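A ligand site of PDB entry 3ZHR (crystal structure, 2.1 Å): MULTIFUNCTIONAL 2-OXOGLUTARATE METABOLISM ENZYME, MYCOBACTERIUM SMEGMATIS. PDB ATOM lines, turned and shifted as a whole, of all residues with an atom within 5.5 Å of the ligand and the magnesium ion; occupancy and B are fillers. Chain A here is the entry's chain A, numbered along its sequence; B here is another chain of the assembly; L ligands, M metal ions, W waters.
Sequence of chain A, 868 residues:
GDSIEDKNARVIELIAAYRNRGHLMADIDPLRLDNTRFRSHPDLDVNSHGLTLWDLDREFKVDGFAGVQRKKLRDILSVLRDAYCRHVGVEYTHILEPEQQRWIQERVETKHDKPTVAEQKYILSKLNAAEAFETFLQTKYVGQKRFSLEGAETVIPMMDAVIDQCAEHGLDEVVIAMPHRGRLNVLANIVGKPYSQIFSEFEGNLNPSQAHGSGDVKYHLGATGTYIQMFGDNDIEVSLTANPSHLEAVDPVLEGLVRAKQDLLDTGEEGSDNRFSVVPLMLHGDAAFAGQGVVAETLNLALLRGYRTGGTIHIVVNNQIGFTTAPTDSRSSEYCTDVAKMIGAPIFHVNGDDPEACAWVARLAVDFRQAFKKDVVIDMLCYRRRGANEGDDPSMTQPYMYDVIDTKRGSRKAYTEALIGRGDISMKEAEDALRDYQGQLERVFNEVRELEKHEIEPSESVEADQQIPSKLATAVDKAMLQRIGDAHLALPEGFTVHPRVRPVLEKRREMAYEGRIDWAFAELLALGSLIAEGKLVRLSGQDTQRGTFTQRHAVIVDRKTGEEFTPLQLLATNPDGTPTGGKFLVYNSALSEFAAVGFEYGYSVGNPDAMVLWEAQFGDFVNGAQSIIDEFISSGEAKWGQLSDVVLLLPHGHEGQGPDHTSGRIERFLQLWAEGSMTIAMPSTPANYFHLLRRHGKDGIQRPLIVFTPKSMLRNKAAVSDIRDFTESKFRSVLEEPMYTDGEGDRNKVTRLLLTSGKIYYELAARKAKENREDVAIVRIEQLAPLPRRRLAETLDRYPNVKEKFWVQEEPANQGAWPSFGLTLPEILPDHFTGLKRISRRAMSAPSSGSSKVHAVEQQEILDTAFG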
ATOM      1  N   ARG A 181      17.756  -6.392  19.981  1.00  0.00           N
ATOM      2  CA  ARG A 181      16.453  -6.543  19.290  1.00  0.00           C
ATOM      3  C   ARG A 181      16.581  -6.899  17.790  1.00  0.00           C
ATOM      4  O   ARG A 181      16.973  -6.075  16.980  1.00  0.00           O
ATOM      5  CB  ARG A 181      15.558  -5.316  19.486  1.00  0.00           C
ATOM      6  CG  ARG A 181      14.074  -5.643  19.403  1.00  0.00           C
ATOM      7  CD  ARG A 181      13.175  -4.453  19.734  1.00  0.00           C
ATOM      8  NE  ARG A 181      13.258  -4.057  21.150  1.00  0.00           N
ATOM      9  CZ  ARG A 181      12.718  -4.735  22.154  1.00  0.00           C
ATOM     10  NH1 ARG A 181      12.030  -5.847  21.919  1.00  0.00           N
ATOM     11  NH2 ARG A 181      12.817  -4.278  23.393  1.00  0.00           N
ATOM     12  N   SER A 245      26.011  -5.251  26.566  1.00  0.00           N
ATOM     13  CA  SER A 245      24.602  -4.910  26.739  1.00  0.00           C
ATOM     14  C   SER A 245      24.454  -3.388  26.903  1.00  0.00           C
ATOM     15  O   SER A 245      23.343  -2.897  26.756  1.00  0.00           O
ATOM     16  CB  SER A 245      23.974  -5.661  27.914  1.00  0.00           C
ATOM     17  OG  SER A 245      23.948  -7.058  27.716  1.00  0.00           O
ATOM     18  N   HIS A 246      25.567  -2.644  27.184  1.00  0.00           N
ATOM     19  CA  HIS A 246      25.566  -1.165  27.325  1.00  0.00           C
ATOM     20  C   HIS A 246      25.169  -0.565  26.020  1.00  0.00           C
ATOM     21  O   HIS A 246      25.965  -0.588  25.071  1.00  0.00           O
ATOM     22  CB  HIS A 246      26.953  -0.622  27.764  1.00  0.00           C
ATOM     23  CG  HIS A 246      27.319  -1.029  29.153  1.00  0.00           C
ATOM     24  ND1 HIS A 246      27.272  -2.346  29.552  1.00  0.00           N
ATOM     25  CD2 HIS A 246      27.734  -0.276  30.189  1.00  0.00           C
ATOM     26  CE1 HIS A 246      27.615  -2.356  30.834  1.00  0.00           C
ATOM     27  NE2 HIS A 246      27.933  -1.127  31.256  1.00  0.00           N
ATOM     28  N   LEU A 247      23.896  -0.111  25.944  1.00  0.00           N
ATOM     29  CA  LEU A 247      23.296   0.443  24.732  1.00  0.00           C
ATOM     30  C   LEU A 247      24.065   1.647  24.261  1.00  0.00           C
ATOM     31  O   LEU A 247      24.467   2.471  25.080  1.00  0.00           O
ATOM     32  CB  LEU A 247      21.821   0.823  24.984  1.00  0.00           C
ATOM     33  CG  LEU A 247      20.853  -0.338  25.390  1.00  0.00           C
ATOM     34  CD1 LEU A 247      19.536   0.188  25.882  1.00  0.00           C
ATOM     35  CD2 LEU A 247      20.615  -1.313  24.246  1.00  0.00           C
ATOM     36  N   GLY A 285      17.855   2.056  19.447  1.00  0.00           N
ATOM     37  CA  GLY A 285      16.529   2.101  20.046  1.00  0.00           C
ATOM     38  C   GLY A 285      16.227   3.567  20.313  1.00  0.00           C
ATOM     39  O   GLY A 285      17.160   4.358  20.477  1.00  0.00           O
ATOM     40  N   ASP A 286      14.941   3.948  20.345  1.00  0.00           N
ATOM     41  CA  ASP A 286      14.513   5.334  20.545  1.00  0.00           C
ATOM     42  C   ASP A 286      14.919   5.917  21.889  1.00  0.00           C
ATOM     43  O   ASP A 286      15.317   7.078  21.922  1.00  0.00           O
ATOM     44  CB  ASP A 286      12.982   5.476  20.370  1.00  0.00           C
ATOM     45  CG  ASP A 286      12.143   4.484  21.166  1.00  0.00           C
ATOM     46  OD1 ASP A 286      12.280   3.262  20.933  1.00  0.00           O
ATOM     47  OD2 ASP A 286      11.333   4.937  22.004  1.00  0.00           O
ATOM     48  N   ALA A 287      14.798   5.154  22.992  1.00  0.00           N
ATOM     49  CA  ALA A 287      15.132   5.737  24.300  1.00  0.00           C
ATOM     50  C   ALA A 287      16.640   5.914  24.456  1.00  0.00           C
ATOM     51  O   ALA A 287      17.073   6.953  24.941  1.00  0.00           O
ATOM     52  CB  ALA A 287      14.556   4.897  25.461  1.00  0.00           C
ATOM     53  N   ALA A 288      17.430   4.956  23.988  1.00  0.00           N
ATOM     54  CA  ALA A 288      18.888   4.989  24.099  1.00  0.00           C
ATOM     55  C   ALA A 288      19.500   6.066  23.205  1.00  0.00           C
ATOM     56  O   ALA A 288      20.465   6.709  23.623  1.00  0.00           O
ATOM     57  CB  ALA A 288      19.482   3.626  23.769  1.00  0.00           C
ATOM     58  N   PHE A 289      18.928   6.292  22.003  1.00  0.00           N
ATOM     59  CA  PHE A 289      19.421   7.297  21.051  1.00  0.00           C
ATOM     60  C   PHE A 289      19.313   8.699  21.617  1.00  0.00           C
ATOM     61  O   PHE A 289      20.188   9.523  21.368  1.00  0.00           O
ATOM     62  CB  PHE A 289      18.673   7.201  19.686  1.00  0.00           C
ATOM     63  CG  PHE A 289      19.405   7.859  18.545  1.00  0.00           C
ATOM     64  CD1 PHE A 289      20.586   7.316  18.030  1.00  0.00           C
ATOM     65  CD2 PHE A 289      18.913   9.023  17.954  1.00  0.00           C
ATOM     66  CE1 PHE A 289      21.239   7.918  16.948  1.00  0.00           C
ATOM     67  CE2 PHE A 289      19.574   9.619  16.882  1.00  0.00           C
ATOM     68  CZ  PHE A 289      20.719   9.056  16.371  1.00  0.00           C
ATOM     69  N   GLN A 292      21.668   8.666  25.676  1.00  0.00           N
ATOM     70  CA  GLN A 292      23.091   8.327  25.834  1.00  0.00           C
ATOM     71  C   GLN A 292      23.996   9.390  25.200  1.00  0.00           C
ATOM     72  O   GLN A 292      23.921   9.640  24.003  1.00  0.00           O
ATOM     73  CB  GLN A 292      23.370   6.920  25.291  1.00  0.00           C
ATOM     74  CG  GLN A 292      22.740   5.784  26.152  1.00  0.00           C
ATOM     75  CD  GLN A 292      23.468   5.613  27.472  1.00  0.00           C
ATOM     76  OE1 GLN A 292      24.687   5.448  27.503  1.00  0.00           O
ATOM     77  NE2 GLN A 292      22.765   5.649  28.597  1.00  0.00           N
ATOM     78  N   VAL A 317      15.138   2.013  15.633  1.00  0.00           N
ATOM     79  CA  VAL A 317      13.973   1.146  15.758  1.00  0.00           C
ATOM     80  C   VAL A 317      13.127   1.839  16.847  1.00  0.00           C
ATOM     81  O   VAL A 317      13.381   1.661  18.049  1.00  0.00           O
ATOM     82  CB  VAL A 317      14.355  -0.324  16.071  1.00  0.00           C
ATOM     83  CG1 VAL A 317      13.114  -1.202  16.271  1.00  0.00           C
ATOM     84  CG2 VAL A 317      15.232  -0.908  14.940  1.00  0.00           C
ATOM     85  N   ASN A 318      12.211   2.727  16.402  1.00  0.00           N
ATOM     86  CA  ASN A 318      11.427   3.549  17.305  1.00  0.00           C
ATOM     87  C   ASN A 318      10.066   2.920  17.607  1.00  0.00           C
ATOM     88  O   ASN A 318       9.076   3.251  16.957  1.00  0.00           O
ATOM     89  CB  ASN A 318      11.278   4.961  16.705  1.00  0.00           C
ATOM     90  CG  ASN A 318      10.541   5.948  17.570  1.00  0.00           C
ATOM     91  OD1 ASN A 318      10.210   5.675  18.737  1.00  0.00           O
ATOM     92  ND2 ASN A 318      10.300   7.127  17.027  1.00  0.00           N
ATOM     93  N   ASN A 319      10.036   2.046  18.637  1.00  0.00           N
ATOM     94  CA  ASN A 319       8.820   1.339  19.071  1.00  0.00           C
ATOM     95  C   ASN A 319       8.056   2.148  20.145  1.00  0.00           C
ATOM     96  O   ASN A 319       7.110   1.633  20.770  1.00  0.00           O
ATOM     97  CB  ASN A 319       9.134  -0.062  19.561  1.00  0.00           C
ATOM     98  CG  ASN A 319      10.242  -0.155  20.586  1.00  0.00           C
ATOM     99  OD1 ASN A 319      10.532   0.804  21.286  1.00  0.00           O
ATOM    100  ND2 ASN A 319      10.869  -1.328  20.688  1.00  0.00           N
ATOM    101  N   GLN A 320       8.488   3.431  20.356  1.00  0.00           N
ATOM    102  CA  GLN A 320       7.801   4.461  21.174  1.00  0.00           C
ATOM    103  C   GLN A 320       7.659   4.053  22.637  1.00  0.00           C
ATOM    104  O   GLN A 320       6.736   4.477  23.342  1.00  0.00           O
ATOM    105  CB  GLN A 320       6.399   4.767  20.545  1.00  0.00           C
ATOM    106  CG  GLN A 320       6.482   5.022  19.019  1.00  0.00           C
ATOM    107  CD  GLN A 320       5.122   5.161  18.364  1.00  0.00           C
ATOM    108  OE1 GLN A 320       4.401   6.128  18.596  1.00  0.00           O
ATOM    109  NE2 GLN A 320       4.741   4.218  17.505  1.00  0.00           N
ATOM    110  N   ILE A 321       8.638   3.280  23.118  1.00  0.00           N
ATOM    111  CA  ILE A 321       8.695   2.792  24.499  1.00  0.00           C
ATOM    112  C   ILE A 321      10.145   2.445  24.798  1.00  0.00           C
ATOM    113  O   ILE A 321      10.921   2.092  23.881  1.00  0.00           O
ATOM    114  CB  ILE A 321       7.705   1.588  24.739  1.00  0.00           C
ATOM    115  CG1 ILE A 321       7.501   1.304  26.273  1.00  0.00           C
ATOM    116  CG2 ILE A 321       8.105   0.307  23.927  1.00  0.00           C
ATOM    117  CD1 ILE A 321       6.336   0.394  26.623  1.00  0.00           C
ATOM    118  N   GLY A 322      10.495   2.617  26.053  1.00  0.00           N
ATOM    119  CA  GLY A 322      11.826   2.294  26.556  1.00  0.00           C
ATOM    120  C   GLY A 322      11.667   1.477  27.827  1.00  0.00           C
ATOM    121  O   GLY A 322      11.567   2.056  28.923  1.00  0.00           O
ATOM    122  N   PHE A 323      11.540   0.138  27.678  1.00  0.00           N
ATOM    123  CA  PHE A 323      11.331  -0.829  28.775  1.00  0.00           C
ATOM    124  C   PHE A 323       9.898  -0.598  29.331  1.00  0.00           C
ATOM    125  O   PHE A 323       8.938  -1.108  28.749  1.00  0.00           O
ATOM    126  CB  PHE A 323      12.458  -0.698  29.847  1.00  0.00           C
ATOM    127  CG  PHE A 323      12.744  -1.944  30.676  1.00  0.00           C
ATOM    128  CD1 PHE A 323      13.626  -2.909  30.235  1.00  0.00           C
ATOM    129  CD2 PHE A 323      12.076  -2.158  31.873  1.00  0.00           C
ATOM    130  CE1 PHE A 323      13.886  -4.047  31.005  1.00  0.00           C
ATOM    131  CE2 PHE A 323      12.313  -3.316  32.636  1.00  0.00           C
ATOM    132  CZ  PHE A 323      13.210  -4.255  32.182  1.00  0.00           C
ATOM    133  N   ARG A 384       6.376  -2.545  19.831  1.00  0.00           N
ATOM    134  CA  ARG A 384       7.012  -3.682  20.463  1.00  0.00           C
ATOM    135  C   ARG A 384       5.873  -4.587  20.933  1.00  0.00           C
ATOM    136  O   ARG A 384       5.206  -4.253  21.917  1.00  0.00           O
ATOM    137  CB  ARG A 384       7.898  -3.141  21.629  1.00  0.00           C
ATOM    138  CG  ARG A 384       8.846  -4.138  22.293  1.00  0.00           C
ATOM    139  CD  ARG A 384       9.258  -3.642  23.686  1.00  0.00           C
ATOM    140  NE  ARG A 384       8.131  -3.723  24.609  1.00  0.00           N
ATOM    141  CZ  ARG A 384       8.097  -3.226  25.841  1.00  0.00           C
ATOM    142  NH1 ARG A 384       9.151  -2.579  26.335  1.00  0.00           N
ATOM    143  NH2 ARG A 384       7.010  -3.346  26.585  1.00  0.00           N
ATOM    144  N   GLN B 542      16.067   4.142  36.062  1.00  0.00           N
ATOM    145  CA  GLN B 542      15.428   3.584  34.887  1.00  0.00           C
ATOM    146  C   GLN B 542      14.347   2.578  35.303  1.00  0.00           C
ATOM    147  O   GLN B 542      14.628   1.623  36.055  1.00  0.00           O
ATOM    148  CB  GLN B 542      16.497   2.943  33.984  1.00  0.00           C
ATOM    149  CG  GLN B 542      17.279   3.992  33.156  1.00  0.00           C
ATOM    150  CD  GLN B 542      18.608   3.482  32.751  1.00  0.00           C
ATOM    151  OE1 GLN B 542      18.828   2.261  32.646  1.00  0.00           O
ATOM    152  NE2 GLN B 542      19.561   4.383  32.603  1.00  0.00           N
ATOM    153  N   ASP B 543      13.083   2.889  34.919  1.00  0.00           N
ATOM    154  CA  ASP B 543      11.904   2.044  35.193  1.00  0.00           C
ATOM    155  C   ASP B 543      11.673   1.815  36.704  1.00  0.00           C
ATOM    156  O   ASP B 543      11.066   0.810  37.098  1.00  0.00           O
ATOM    157  CB  ASP B 543      12.064   0.707  34.448  1.00  0.00           C
ATOM    158  CG  ASP B 543      12.348   0.974  32.982  1.00  0.00           C
ATOM    159  OD1 ASP B 543      11.419   1.483  32.282  1.00  0.00           O
ATOM    160  OD2 ASP B 543      13.512   0.789  32.564  1.00  0.00           O
ATOM    161  N   LEU B 591      17.107   7.479  29.666  1.00  0.00           N
ATOM    162  CA  LEU B 591      18.082   6.410  29.511  1.00  0.00           C
ATOM    163  C   LEU B 591      19.496   6.984  29.544  1.00  0.00           C
ATOM    164  O   LEU B 591      20.225   6.937  28.540  1.00  0.00           O
ATOM    165  CB  LEU B 591      17.860   5.605  28.230  1.00  0.00           C
ATOM    166  CG  LEU B 591      18.128   4.114  28.359  1.00  0.00           C
ATOM    167  CD1 LEU B 591      17.509   3.372  27.201  1.00  0.00           C
ATOM    168  CD2 LEU B 591      19.664   3.784  28.502  1.00  0.00           C
ATOM    169  N   GLU B 593      22.971   7.506  32.524  1.00  0.00           N
ATOM    170  CA  GLU B 593      23.556   7.175  33.816  1.00  0.00           C
ATOM    171  C   GLU B 593      24.329   8.391  34.279  1.00  0.00           C
ATOM    172  O   GLU B 593      24.048   8.910  35.348  1.00  0.00           O
ATOM    173  CB  GLU B 593      24.441   5.904  33.755  1.00  0.00           C
ATOM    174  CG  GLU B 593      23.632   4.633  33.661  1.00  0.00           C
ATOM    175  CD  GLU B 593      23.147   4.260  32.260  1.00  0.00           C
ATOM    176  OE1 GLU B 593      23.810   4.644  31.269  1.00  0.00           O
ATOM    177  OE2 GLU B 593      22.109   3.581  32.171  1.00  0.00           O
ATOM    178  N   GLN B 617      19.565   0.275  36.592  1.00  0.00           N
ATOM    179  CA  GLN B 617      18.719  -0.806  36.099  1.00  0.00           C
ATOM    180  C   GLN B 617      19.327  -2.140  36.590  1.00  0.00           C
ATOM    181  O   GLN B 617      18.631  -3.028  37.128  1.00  0.00           O
ATOM    182  CB  GLN B 617      18.552  -0.742  34.562  1.00  0.00           C
ATOM    183  CG  GLN B 617      17.090  -0.804  34.212  1.00  0.00           C
ATOM    184  CD  GLN B 617      16.736  -1.657  33.042  1.00  0.00           C
ATOM    185  OE1 GLN B 617      17.438  -2.595  32.667  1.00  0.00           O
ATOM    186  NE2 GLN B 617      15.605  -1.384  32.474  1.00  0.00           N
ATOM    187  N   PHE B 621      25.648  -0.996  34.787  1.00  0.00           N
ATOM    188  CA  PHE B 621      25.536   0.178  33.936  1.00  0.00           C
ATOM    189  C   PHE B 621      26.001   1.463  34.618  1.00  0.00           C
ATOM    190  O   PHE B 621      26.158   2.471  33.932  1.00  0.00           O
ATOM    191  CB  PHE B 621      24.096   0.332  33.404  1.00  0.00           C
ATOM    192  CG  PHE B 621      23.658  -0.878  32.624  1.00  0.00           C
ATOM    193  CD1 PHE B 621      24.359  -1.285  31.494  1.00  0.00           C
ATOM    194  CD2 PHE B 621      22.573  -1.628  33.035  1.00  0.00           C
ATOM    195  CE1 PHE B 621      23.983  -2.433  30.795  1.00  0.00           C
ATOM    196  CE2 PHE B 621      22.197  -2.790  32.338  1.00  0.00           C
ATOM    197  CZ  PHE B 621      22.899  -3.182  31.217  1.00  0.00           C
ATOM    198  N   HIS B 661      24.980  -8.063  33.476  1.00  0.00           N
ATOM    199  CA  HIS B 661      23.790  -8.205  34.328  1.00  0.00           C
ATOM    200  C   HIS B 661      24.195  -9.034  35.554  1.00  0.00           C
ATOM    201  O   HIS B 661      23.437  -9.859  36.049  1.00  0.00           O
ATOM    202  CB  HIS B 661      22.633  -8.826  33.544  1.00  0.00           C
ATOM    203  CG  HIS B 661      22.216  -8.006  32.369  1.00  0.00           C
ATOM    204  ND1 HIS B 661      21.197  -7.076  32.458  1.00  0.00           N
ATOM    205  CD2 HIS B 661      22.710  -7.970  31.096  1.00  0.00           C
ATOM    206  CE1 HIS B 661      21.101  -6.520  31.263  1.00  0.00           C
ATOM    207  NE2 HIS B 661      21.994  -7.006  30.414  1.00  0.00           N
HETATM  208  N1  LIG L   1      21.781   1.556  30.286  1.00  0.00           N
HETATM  209  C1  LIG L   1      22.609   1.141  29.333  1.00  0.00           C
HETATM  210  C2  LIG L   1      23.785   1.990  28.957  1.00  0.00           C
HETATM  211  N2  LIG L   1      22.400  -0.012  28.717  1.00  0.00           N
HETATM  212  C3  LIG L   1      21.374  -0.807  29.060  1.00  0.00           C
HETATM  213  N3  LIG L   1      21.276  -2.020  28.456  1.00  0.00           N
HETATM  214  C4  LIG L   1      20.462  -0.399  30.049  1.00  0.00           C
HETATM  215  C5  LIG L   1      20.738   0.816  30.665  1.00  0.00           C
HETATM  216  C6  LIG L   1      19.242  -1.191  30.481  1.00  0.00           C
HETATM  217  N4  LIG L   1      18.196  -1.273  29.430  1.00  0.00           N
HETATM  218  C7  LIG L   1      18.050  -2.372  28.746  1.00  0.00           C
HETATM  219  S1  LIG L   1      16.748  -2.258  27.638  1.00  0.00           S
HETATM  220  C8  LIG L   1      16.374  -0.624  28.204  1.00  0.00           C
HETATM  221  C9  LIG L   1      17.305  -0.313  29.148  1.00  0.00           C
HETATM  222  C10 LIG L   1      17.179   1.039  29.850  1.00  0.00           C
HETATM  223  C11 LIG L   1      15.322   0.250  27.556  1.00  0.00           C
HETATM  224  C12 LIG L   1      15.778   0.417  26.082  1.00  0.00           C
HETATM  225  O1  LIG L   1      14.934   1.285  25.314  1.00  0.00           O
HETATM  226  P1  LIG L   1      15.162   1.509  23.744  1.00  0.00           P
HETATM  227  O2  LIG L   1      16.479   2.211  23.517  1.00  0.00           O
HETATM  228  O3  LIG L   1      13.981   2.432  23.187  1.00  0.00           O
HETATM  229  O4  LIG L   1      15.233   0.064  23.023  1.00  0.00           O
HETATM  230  P2  LIG L   1      14.154  -1.023  22.893  1.00  0.00           P
HETATM  231  O5  LIG L   1      14.332  -2.106  24.044  1.00  0.00           O
HETATM  232  O6  LIG L   1      12.845  -0.291  23.024  1.00  0.00           O
HETATM  233  O7  LIG L   1      14.386  -1.635  21.432  1.00  0.00           O
HETATM  234 MG    MG M   1      12.289   1.580  22.219  1.00  0.00          MG
HETATM  235  O   HOH W   1      14.193   2.667  30.636  1.00  0.00           O
HETATM  236  O   HOH W   2      26.209   2.885  31.316  1.00  0.00           O
HETATM  237  O   HOH W   3      13.639  -2.652  26.349  1.00  0.00           O
HETATM  238  O   HOH W   4      11.419  -1.276  25.203  1.00  0.00           O
HETATM  239  O   HOH W   5      13.302   0.834  20.574  1.00  0.00           O
HETATM  240  O   HOH W   6      17.264  -2.051  23.805  1.00  0.00           O
HETATM  241  O   HOH W   7      18.319   0.360  22.322  1.00  0.00           O
HETATM  242  O   HOH W   8      16.846  -1.525  20.687  1.00  0.00           O
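Within 4 Å of the magnesium ion: Asp 286, Asn 319 and Ile 321. The nearest printed residue that does not touch the magnesium ion is Val 317 (4.3 Å).
The magnesium ion is bound by water W5 (2.1 Å), an oxygen (O6) of the ligand (2.1 Å), the side-chain carboxylate of Asp 286 (2.1 Å), an oxygen (O3) of the ligand (2.1 Å), the side-chain amide oxygen of Asn 319 (2.1 Å) and the backbone carbonyl oxygen of Ile 321 (2.2 Å). The magnesium ion has six donor atoms within binding distance.
Water W5 lies within hydrogen-bond range of O of Val 317, O7 of the ligand and ND2 of Asn 319. Water W3 lies within hydrogen-bond range of O5 of the ligand (2.5 Å) and NH2 of Arg 181 (3.5 Å). Water W4 lies within hydrogen-bond range of NH1 of Arg 384, N of Phe 323 and O5 of the ligand. Water W7 bridges O2 of the ligand (2.9 Å) and N of Gly 285 (3.4 Å). Water W1 lies within hydrogen-bond range of the side-chain carboxylate of Asp 543 of chain B and the backbone carbonyl oxygen of Gly 322. Water W2 bridges the backbone carbonyl oxygen of Phe 621 of chain B and the side-chain carboxylate of Glu 593 of chain B.
The backbone NH (N) of Asp 286 lies close to an oxygen (O3) of the ligand, at 3.4 Å. NE of Arg 181 lies within salt-bridge range of O7 of the ligand (2.7 Å). N1 of the ligand is in hydrogen-bond range of OE2 of Glu 593 of chain B. O of Ser 245 sits at hydrogen-bond distance from N3 of the ligand, at 2.8 Å. O2 of the ligand sits at hydrogen-bond distance from N of Ala 287 (3.4 Å). O2 of the ligand is in hydrogen-bond range of N of Ala 288 (2.9 Å). A nitrogen (N2) of the ligand lies within hydrogen-bond range of the backbone NH of Leu 247, at 3.2 Å.
Merely in contact with the ligand: Gln 542 of chain B, Gln 617 of chain B, Phe 621 of chain B, Gly 285, Gly 322, Leu 591 of chain B, His 246, Phe 323 and Gln 292. Hydrophobic or aromatic side chains that line the ligand: Leu 247, Ala 287, Ala 288, Phe 323, Leu 591 of chain B and Phe 621 of chain B. The nearest printed residue that does not touch the ligand is Asp 543 of chain B (4.6 Å).
The side-chain amide nitrogen of Gln 542 of chain B sits at hydrogen-bond distance from the side-chain carboxylate of Glu 593 of chain B. The side-chain amide nitrogen of Gln 292 lies within hydrogen-bond range of the side-chain carboxylate of Glu 593 of chain B (3.0 Å). The side-chain hydroxyl (OG) of Ser 245 sits at hydrogen-bond distance from a ring nitrogen (NE2) of His 661 of chain B (3.3 Å). NE2 of Gln 617 of chain B is in hydrogen-bond range of OD2 of Asp 543 of chain B. NE2 of Gln 292 is in hydrogen-bond range of O of Leu 591 of chain B (2.8 Å). The backbone carbonyl oxygen of Phe 323 is in hydrogen-bond range of the guanidinium group of Arg 384, 2.8 Å away.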
